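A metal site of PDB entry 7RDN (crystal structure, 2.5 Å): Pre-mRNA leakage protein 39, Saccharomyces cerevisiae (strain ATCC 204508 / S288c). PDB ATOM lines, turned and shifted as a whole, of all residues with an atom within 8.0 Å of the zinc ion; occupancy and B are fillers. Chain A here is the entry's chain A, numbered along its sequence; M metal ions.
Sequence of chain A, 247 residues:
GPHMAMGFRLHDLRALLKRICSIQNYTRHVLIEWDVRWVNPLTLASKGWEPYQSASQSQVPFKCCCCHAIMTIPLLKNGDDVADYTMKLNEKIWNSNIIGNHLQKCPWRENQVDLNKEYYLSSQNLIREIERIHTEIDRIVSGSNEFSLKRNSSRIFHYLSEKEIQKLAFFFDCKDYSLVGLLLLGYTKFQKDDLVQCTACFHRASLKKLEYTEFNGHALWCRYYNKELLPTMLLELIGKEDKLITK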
ATOM      1  N   GLN A  24     -25.486 -25.226  15.892  1.00  0.00           N
ATOM      2  CA  GLN A  24     -26.034 -26.019  14.806  1.00  0.00           C
ATOM      3  C   GLN A  24     -26.688 -27.288  15.332  1.00  0.00           C
ATOM      4  O   GLN A  24     -27.742 -27.701  14.838  1.00  0.00           O
ATOM      5  CB  GLN A  24     -24.947 -26.355  13.792  1.00  0.00           C
ATOM      6  CG  GLN A  24     -24.376 -25.157  13.056  1.00  0.00           C
ATOM      7  CD  GLN A  24     -25.401 -24.452  12.174  1.00  0.00           C
ATOM      8  OE1 GLN A  24     -26.401 -23.937  12.661  1.00  0.00           O
ATOM      9  NE2 GLN A  24     -25.146 -24.431  10.868  1.00  0.00           N
ATOM     10  N   TYR A 119     -11.812 -17.058  10.894  1.00  0.00           N
ATOM     11  CA  TYR A 119     -12.789 -18.003  10.377  1.00  0.00           C
ATOM     12  C   TYR A 119     -12.746 -18.138   8.863  1.00  0.00           C
ATOM     13  O   TYR A 119     -12.605 -19.248   8.342  1.00  0.00           O
ATOM     14  CB  TYR A 119     -14.208 -17.592  10.812  1.00  0.00           C
ATOM     15  CG  TYR A 119     -15.285 -18.545  10.355  1.00  0.00           C
ATOM     16  CD1 TYR A 119     -15.550 -19.704  11.066  1.00  0.00           C
ATOM     17  CD2 TYR A 119     -16.021 -18.292   9.203  1.00  0.00           C
ATOM     18  CE1 TYR A 119     -16.523 -20.582  10.662  1.00  0.00           C
ATOM     19  CE2 TYR A 119     -17.001 -19.170   8.783  1.00  0.00           C
ATOM     20  CZ  TYR A 119     -17.253 -20.313   9.519  1.00  0.00           C
ATOM     21  OH  TYR A 119     -18.230 -21.184   9.104  1.00  0.00           O
ATOM     22  N   LEU A 185     -13.753 -29.535  -0.281  1.00  0.00           N
ATOM     23  CA  LEU A 185     -15.053 -28.952   0.019  1.00  0.00           C
ATOM     24  C   LEU A 185     -15.265 -28.708   1.512  1.00  0.00           C
ATOM     25  O   LEU A 185     -16.340 -28.248   1.898  1.00  0.00           O
ATOM     26  CB  LEU A 185     -16.169 -29.837  -0.520  1.00  0.00           C
ATOM     27  CG  LEU A 185     -16.267 -29.945  -2.044  1.00  0.00           C
ATOM     28  CD1 LEU A 185     -17.349 -30.927  -2.430  1.00  0.00           C
ATOM     29  CD2 LEU A 185     -16.542 -28.579  -2.664  1.00  0.00           C
ATOM     30  N   GLY A 186     -14.274 -29.022   2.352  1.00  0.00           N
ATOM     31  CA  GLY A 186     -14.349 -28.754   3.776  1.00  0.00           C
ATOM     32  C   GLY A 186     -15.002 -29.837   4.604  1.00  0.00           C
ATOM     33  O   GLY A 186     -15.217 -29.620   5.804  1.00  0.00           O
ATOM     34  N   TYR A 187     -15.313 -30.977   4.014  1.00  0.00           N
ATOM     35  CA  TYR A 187     -16.052 -32.016   4.711  1.00  0.00           C
ATOM     36  C   TYR A 187     -15.135 -32.993   5.439  1.00  0.00           C
ATOM     37  O   TYR A 187     -13.924 -33.023   5.235  1.00  0.00           O
ATOM     38  CB  TYR A 187     -16.939 -32.771   3.710  1.00  0.00           C
ATOM     39  CG  TYR A 187     -18.167 -32.014   3.301  1.00  0.00           C
ATOM     40  CD1 TYR A 187     -18.222 -31.343   2.085  1.00  0.00           C
ATOM     41  CD2 TYR A 187     -19.280 -31.959   4.121  1.00  0.00           C
ATOM     42  CE1 TYR A 187     -19.344 -30.657   1.699  1.00  0.00           C
ATOM     43  CE2 TYR A 187     -20.415 -31.272   3.741  1.00  0.00           C
ATOM     44  CZ  TYR A 187     -20.437 -30.621   2.536  1.00  0.00           C
ATOM     45  OH  TYR A 187     -21.563 -29.922   2.153  1.00  0.00           O
ATOM     46  N   GLN A 197     -19.970 -34.487   7.368  1.00  0.00           N
ATOM     47  CA  GLN A 197     -20.236 -33.229   8.055  1.00  0.00           C
ATOM     48  C   GLN A 197     -19.191 -32.195   7.682  1.00  0.00           C
ATOM     49  O   GLN A 197     -18.007 -32.514   7.560  1.00  0.00           O
ATOM     50  CB  GLN A 197     -20.258 -33.435   9.562  1.00  0.00           C
ATOM     51  CG  GLN A 197     -20.870 -32.281  10.348  1.00  0.00           C
ATOM     52  CD  GLN A 197     -20.844 -32.536  11.840  1.00  0.00           C
ATOM     53  OE1 GLN A 197     -21.884 -32.573  12.497  1.00  0.00           O
ATOM     54  NE2 GLN A 197     -19.644 -32.702  12.383  1.00  0.00           N
ATOM     55  N   CYS A 198     -19.622 -30.945   7.513  1.00  0.00           N
ATOM     56  CA  CYS A 198     -18.697 -29.860   7.259  1.00  0.00           C
ATOM     57  C   CYS A 198     -18.008 -29.420   8.537  1.00  0.00           C
ATOM     58  O   CYS A 198     -18.599 -29.412   9.621  1.00  0.00           O
ATOM     59  CB  CYS A 198     -19.403 -28.664   6.641  1.00  0.00           C
ATOM     60  SG  CYS A 198     -18.333 -27.211   6.501  1.00  0.00           S
ATOM     61  N   THR A 199     -16.740 -29.030   8.404  1.00  0.00           N
ATOM     62  CA  THR A 199     -15.934 -28.666   9.563  1.00  0.00           C
ATOM     63  C   THR A 199     -16.132 -27.221  10.007  1.00  0.00           C
ATOM     64  O   THR A 199     -15.728 -26.872  11.121  1.00  0.00           O
ATOM     65  CB  THR A 199     -14.449 -28.894   9.274  1.00  0.00           C
ATOM     66  OG1 THR A 199     -14.053 -28.140   8.121  1.00  0.00           O
ATOM     67  CG2 THR A 199     -14.171 -30.375   9.034  1.00  0.00           C
ATOM     68  N   ALA A 200     -16.732 -26.363   9.177  1.00  0.00           N
ATOM     69  CA  ALA A 200     -16.863 -24.957   9.498  1.00  0.00           C
ATOM     70  C   ALA A 200     -18.304 -24.487   9.674  1.00  0.00           C
ATOM     71  O   ALA A 200     -18.530 -23.518  10.396  1.00  0.00           O
ATOM     72  CB  ALA A 200     -16.200 -24.088   8.424  1.00  0.00           C
ATOM     73  N   CYS A 201     -19.274 -25.125   9.022  1.00  0.00           N
ATOM     74  CA  CYS A 201     -20.677 -24.820   9.254  1.00  0.00           C
ATOM     75  C   CYS A 201     -21.452 -26.008   9.813  1.00  0.00           C
ATOM     76  O   CYS A 201     -22.570 -25.810  10.306  1.00  0.00           O
ATOM     77  CB  CYS A 201     -21.362 -24.349   7.958  1.00  0.00           C
ATOM     78  SG  CYS A 201     -21.851 -25.677   6.826  1.00  0.00           S
ATOM     79  N   PHE A 202     -20.885 -27.208   9.751  1.00  0.00           N
ATOM     80  CA  PHE A 202     -21.420 -28.389  10.416  1.00  0.00           C
ATOM     81  C   PHE A 202     -22.751 -28.841   9.830  1.00  0.00           C
ATOM     82  O   PHE A 202     -23.517 -29.543  10.506  1.00  0.00           O
ATOM     83  CB  PHE A 202     -21.527 -28.146  11.922  1.00  0.00           C
ATOM     84  CG  PHE A 202     -20.236 -27.682  12.537  1.00  0.00           C
ATOM     85  CD1 PHE A 202     -19.321 -28.604  13.017  1.00  0.00           C
ATOM     86  CD2 PHE A 202     -19.929 -26.333  12.595  1.00  0.00           C
ATOM     87  CE1 PHE A 202     -18.129 -28.174  13.573  1.00  0.00           C
ATOM     88  CE2 PHE A 202     -18.728 -25.913  13.141  1.00  0.00           C
ATOM     89  CZ  PHE A 202     -17.831 -26.835  13.634  1.00  0.00           C
ATOM     90  N   HIS A 203     -23.045 -28.460   8.596  1.00  0.00           N
ATOM     91  CA  HIS A 203     -24.139 -29.084   7.864  1.00  0.00           C
ATOM     92  C   HIS A 203     -23.769 -30.520   7.512  1.00  0.00           C
ATOM     93  O   HIS A 203     -22.595 -30.864   7.374  1.00  0.00           O
ATOM     94  CB  HIS A 203     -24.459 -28.295   6.597  1.00  0.00           C
ATOM     95  CG  HIS A 203     -25.248 -27.047   6.852  1.00  0.00           C
ATOM     96  ND1 HIS A 203     -25.842 -26.317   5.842  1.00  0.00           N
ATOM     97  CD2 HIS A 203     -25.547 -26.388   8.000  1.00  0.00           C
ATOM     98  CE1 HIS A 203     -26.464 -25.272   6.349  1.00  0.00           C
ATOM     99  NE2 HIS A 203     -26.300 -25.294   7.656  1.00  0.00           N
ATOM    100  N   ARG A 204     -24.795 -31.355   7.374  1.00  0.00           N
ATOM    101  CA  ARG A 204     -24.616 -32.771   7.076  1.00  0.00           C
ATOM    102  C   ARG A 204     -25.164 -33.082   5.698  1.00  0.00           C
ATOM    103  O   ARG A 204     -26.269 -32.640   5.352  1.00  0.00           O
ATOM    104  CB  ARG A 204     -25.294 -33.634   8.132  1.00  0.00           C
ATOM    105  CG  ARG A 204     -24.707 -33.465   9.529  1.00  0.00           C
ATOM    106  CD  ARG A 204     -25.525 -34.181  10.582  1.00  0.00           C
ATOM    107  NE  ARG A 204     -25.012 -33.929  11.918  1.00  0.00           N
ATOM    108  CZ  ARG A 204     -25.610 -34.318  13.042  1.00  0.00           C
ATOM    109  NH1 ARG A 204     -26.747 -34.993  13.022  1.00  0.00           N
ATOM    110  NH2 ARG A 204     -25.058 -34.016  14.211  1.00  0.00           N
ATOM    111  N   ASN A 216     -24.882 -27.626  -3.202  1.00  0.00           N
ATOM    112  CA  ASN A 216     -23.989 -27.041  -2.213  1.00  0.00           C
ATOM    113  C   ASN A 216     -24.659 -27.183  -0.855  1.00  0.00           C
ATOM    114  O   ASN A 216     -25.713 -26.588  -0.601  1.00  0.00           O
ATOM    115  CB  ASN A 216     -23.701 -25.581  -2.540  1.00  0.00           C
ATOM    116  CG  ASN A 216     -22.690 -24.953  -1.599  1.00  0.00           C
ATOM    117  OD1 ASN A 216     -22.543 -25.359  -0.447  1.00  0.00           O
ATOM    118  ND2 ASN A 216     -21.966 -23.940  -2.083  1.00  0.00           N
ATOM    119  N   GLY A 217     -24.042 -27.968   0.026  1.00  0.00           N
ATOM    120  CA  GLY A 217     -24.584 -28.245   1.335  1.00  0.00           C
ATOM    121  C   GLY A 217     -24.173 -27.280   2.418  1.00  0.00           C
ATOM    122  O   GLY A 217     -24.469 -27.515   3.594  1.00  0.00           O
ATOM    123  N   HIS A 218     -23.513 -26.183   2.062  1.00  0.00           N
ATOM    124  CA  HIS A 218     -23.005 -25.235   3.049  1.00  0.00           C
ATOM    125  C   HIS A 218     -24.019 -24.113   3.295  1.00  0.00           C
ATOM    126  O   HIS A 218     -24.807 -23.750   2.421  1.00  0.00           O
ATOM    127  CB  HIS A 218     -21.682 -24.631   2.577  1.00  0.00           C
ATOM    128  CG  HIS A 218     -20.583 -25.630   2.416  1.00  0.00           C
ATOM    129  ND1 HIS A 218     -19.886 -26.150   3.481  1.00  0.00           N
ATOM    130  CD2 HIS A 218     -20.052 -26.196   1.305  1.00  0.00           C
ATOM    131  CE1 HIS A 218     -18.981 -27.004   3.041  1.00  0.00           C
ATOM    132  NE2 HIS A 218     -19.060 -27.049   1.722  1.00  0.00           N
ATOM    133  N   ALA A 219     -23.976 -23.577   4.511  1.00  0.00           N
ATOM    134  CA  ALA A 219     -24.711 -22.356   4.812  1.00  0.00           C
ATOM    135  C   ALA A 219     -24.115 -21.180   4.034  1.00  0.00           C
ATOM    136  O   ALA A 219     -22.936 -21.184   3.650  1.00  0.00           O
ATOM    137  CB  ALA A 219     -24.674 -22.067   6.309  1.00  0.00           C
ATOM    138  N   LEU A 220     -24.943 -20.162   3.800  1.00  0.00           N
ATOM    139  CA  LEU A 220     -24.479 -18.991   3.077  1.00  0.00           C
ATOM    140  C   LEU A 220     -23.271 -18.348   3.761  1.00  0.00           C
ATOM    141  O   LEU A 220     -22.430 -17.734   3.096  1.00  0.00           O
ATOM    142  CB  LEU A 220     -25.601 -17.968   2.954  1.00  0.00           C
ATOM    143  CG  LEU A 220     -26.702 -18.289   1.943  1.00  0.00           C
ATOM    144  CD1 LEU A 220     -27.881 -17.340   2.136  1.00  0.00           C
ATOM    145  CD2 LEU A 220     -26.161 -18.184   0.531  1.00  0.00           C
ATOM    146  N   TRP A 221     -23.174 -18.488   5.082  1.00  0.00           N
ATOM    147  CA  TRP A 221     -22.119 -17.872   5.873  1.00  0.00           C
ATOM    148  C   TRP A 221     -20.921 -18.778   6.097  1.00  0.00           C
ATOM    149  O   TRP A 221     -19.990 -18.384   6.805  1.00  0.00           O
ATOM    150  CB  TRP A 221     -22.682 -17.419   7.227  1.00  0.00           C
ATOM    151  CG  TRP A 221     -23.511 -18.467   7.917  1.00  0.00           C
ATOM    152  CD1 TRP A 221     -24.876 -18.551   7.926  1.00  0.00           C
ATOM    153  CD2 TRP A 221     -23.034 -19.566   8.695  1.00  0.00           C
ATOM    154  NE1 TRP A 221     -25.268 -19.646   8.659  1.00  0.00           N
ATOM    155  CE2 TRP A 221     -24.162 -20.284   9.139  1.00  0.00           C
ATOM    156  CE3 TRP A 221     -21.761 -20.026   9.059  1.00  0.00           C
ATOM    157  CZ2 TRP A 221     -24.054 -21.429   9.938  1.00  0.00           C
ATOM    158  CZ3 TRP A 221     -21.661 -21.155   9.836  1.00  0.00           C
ATOM    159  CH2 TRP A 221     -22.805 -21.847  10.269  1.00  0.00           C
ATOM    160  N   CYS A 222     -20.914 -19.979   5.512  1.00  0.00           N
ATOM    161  CA  CYS A 222     -19.824 -20.906   5.763  1.00  0.00           C
ATOM    162  C   CYS A 222     -18.537 -20.455   5.078  1.00  0.00           C
ATOM    163  O   CYS A 222     -18.549 -19.820   4.031  1.00  0.00           O
ATOM    164  CB  CYS A 222     -20.168 -22.318   5.269  1.00  0.00           C
ATOM    165  SG  CYS A 222     -18.832 -23.528   5.569  1.00  0.00           S
ATOM    166  N   ARG A 223     -17.415 -20.821   5.694  1.00  0.00           N
ATOM    167  CA  ARG A 223     -16.112 -20.576   5.088  1.00  0.00           C
ATOM    168  C   ARG A 223     -16.037 -21.144   3.684  1.00  0.00           C
ATOM    169  O   ARG A 223     -15.416 -20.550   2.798  1.00  0.00           O
ATOM    170  CB  ARG A 223     -15.022 -21.190   5.981  1.00  0.00           C
ATOM    171  CG  ARG A 223     -13.600 -21.045   5.455  1.00  0.00           C
ATOM    172  CD  ARG A 223     -12.653 -21.984   6.203  1.00  0.00           C
ATOM    173  NE  ARG A 223     -12.683 -21.771   7.645  1.00  0.00           N
ATOM    174  CZ  ARG A 223     -12.334 -22.678   8.542  1.00  0.00           C
ATOM    175  NH1 ARG A 223     -11.944 -23.886   8.190  1.00  0.00           N
ATOM    176  NH2 ARG A 223     -12.386 -22.365   9.838  1.00  0.00           N
ATOM    177  N   TYR A 224     -16.682 -22.289   3.445  1.00  0.00           N
ATOM    178  CA  TYR A 224     -16.555 -23.023   2.192  1.00  0.00           C
ATOM    179  C   TYR A 224     -17.749 -22.833   1.247  1.00  0.00           C
ATOM    180  O   TYR A 224     -17.863 -23.580   0.276  1.00  0.00           O
ATOM    181  CB  TYR A 224     -16.376 -24.518   2.462  1.00  0.00           C
ATOM    182  CG  TYR A 224     -15.256 -24.858   3.417  1.00  0.00           C
ATOM    183  CD1 TYR A 224     -13.938 -24.671   3.053  1.00  0.00           C
ATOM    184  CD2 TYR A 224     -15.526 -25.395   4.677  1.00  0.00           C
ATOM    185  CE1 TYR A 224     -12.907 -24.990   3.914  1.00  0.00           C
ATOM    186  CE2 TYR A 224     -14.501 -25.717   5.546  1.00  0.00           C
ATOM    187  CZ  TYR A 224     -13.192 -25.521   5.155  1.00  0.00           C
ATOM    188  OH  TYR A 224     -12.162 -25.824   6.010  1.00  0.00           O
ATOM    189  N   TYR A 225     -18.627 -21.862   1.504  1.00  0.00           N
ATOM    190  CA  TYR A 225     -19.827 -21.765   0.691  1.00  0.00           C
ATOM    191  C   TYR A 225     -19.502 -21.628  -0.787  1.00  0.00           C
ATOM    192  O   TYR A 225     -20.149 -22.254  -1.635  1.00  0.00           O
ATOM    193  CB  TYR A 225     -20.709 -20.587   1.120  1.00  0.00           C
ATOM    194  CG  TYR A 225     -21.930 -20.486   0.236  1.00  0.00           C
ATOM    195  CD1 TYR A 225     -22.971 -21.400   0.353  1.00  0.00           C
ATOM    196  CD2 TYR A 225     -22.013 -19.521  -0.752  1.00  0.00           C
ATOM    197  CE1 TYR A 225     -24.083 -21.323  -0.466  1.00  0.00           C
ATOM    198  CE2 TYR A 225     -23.121 -19.442  -1.578  1.00  0.00           C
ATOM    199  CZ  TYR A 225     -24.152 -20.343  -1.427  1.00  0.00           C
ATOM    200  OH  TYR A 225     -25.252 -20.268  -2.251  1.00  0.00           O
HETATM  201 ZN    ZN M   1     -19.936 -25.571   5.513  1.00  0.00          ZN
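N of Cys 198 lies within hydrogen-bond range of O of His 203, at 3.0 Å. O of Cys 201 is in hydrogen-bond range of NE2 of Gln 24, at 3.0 Å. SG of Cys 201 lies close to N of Ala 219, at 3.8 Å. The side-chain sulfur (SG) of Cys 201 sits close to the backbone NH (N) of His 203, 3.5 Å away. The side-chain sulfur (SG) of Cys 222 lies close to the backbone NH (N) of Tyr 224 (3.3 Å). NE2 of His 218 is in hydrogen-bond range of O of Leu 185. N of His 218 sits at hydrogen-bond distance from OD1 of Asn 216 (2.8 Å). SG of Cys 198 lies close to N of Ala 200.
Of the 23 residues printed, 4 come within 4 Å of the zinc ion. The nearest printed residue that does not touch the zinc ion is Tyr 224 (4.5 Å).
The zinc ion is bound by ND1 of His 218 (2.1 Å), SG of Cys 222 (2.3 Å), SG of Cys 201 (2.3 Å) and SG of Cys 198 (2.5 Å).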
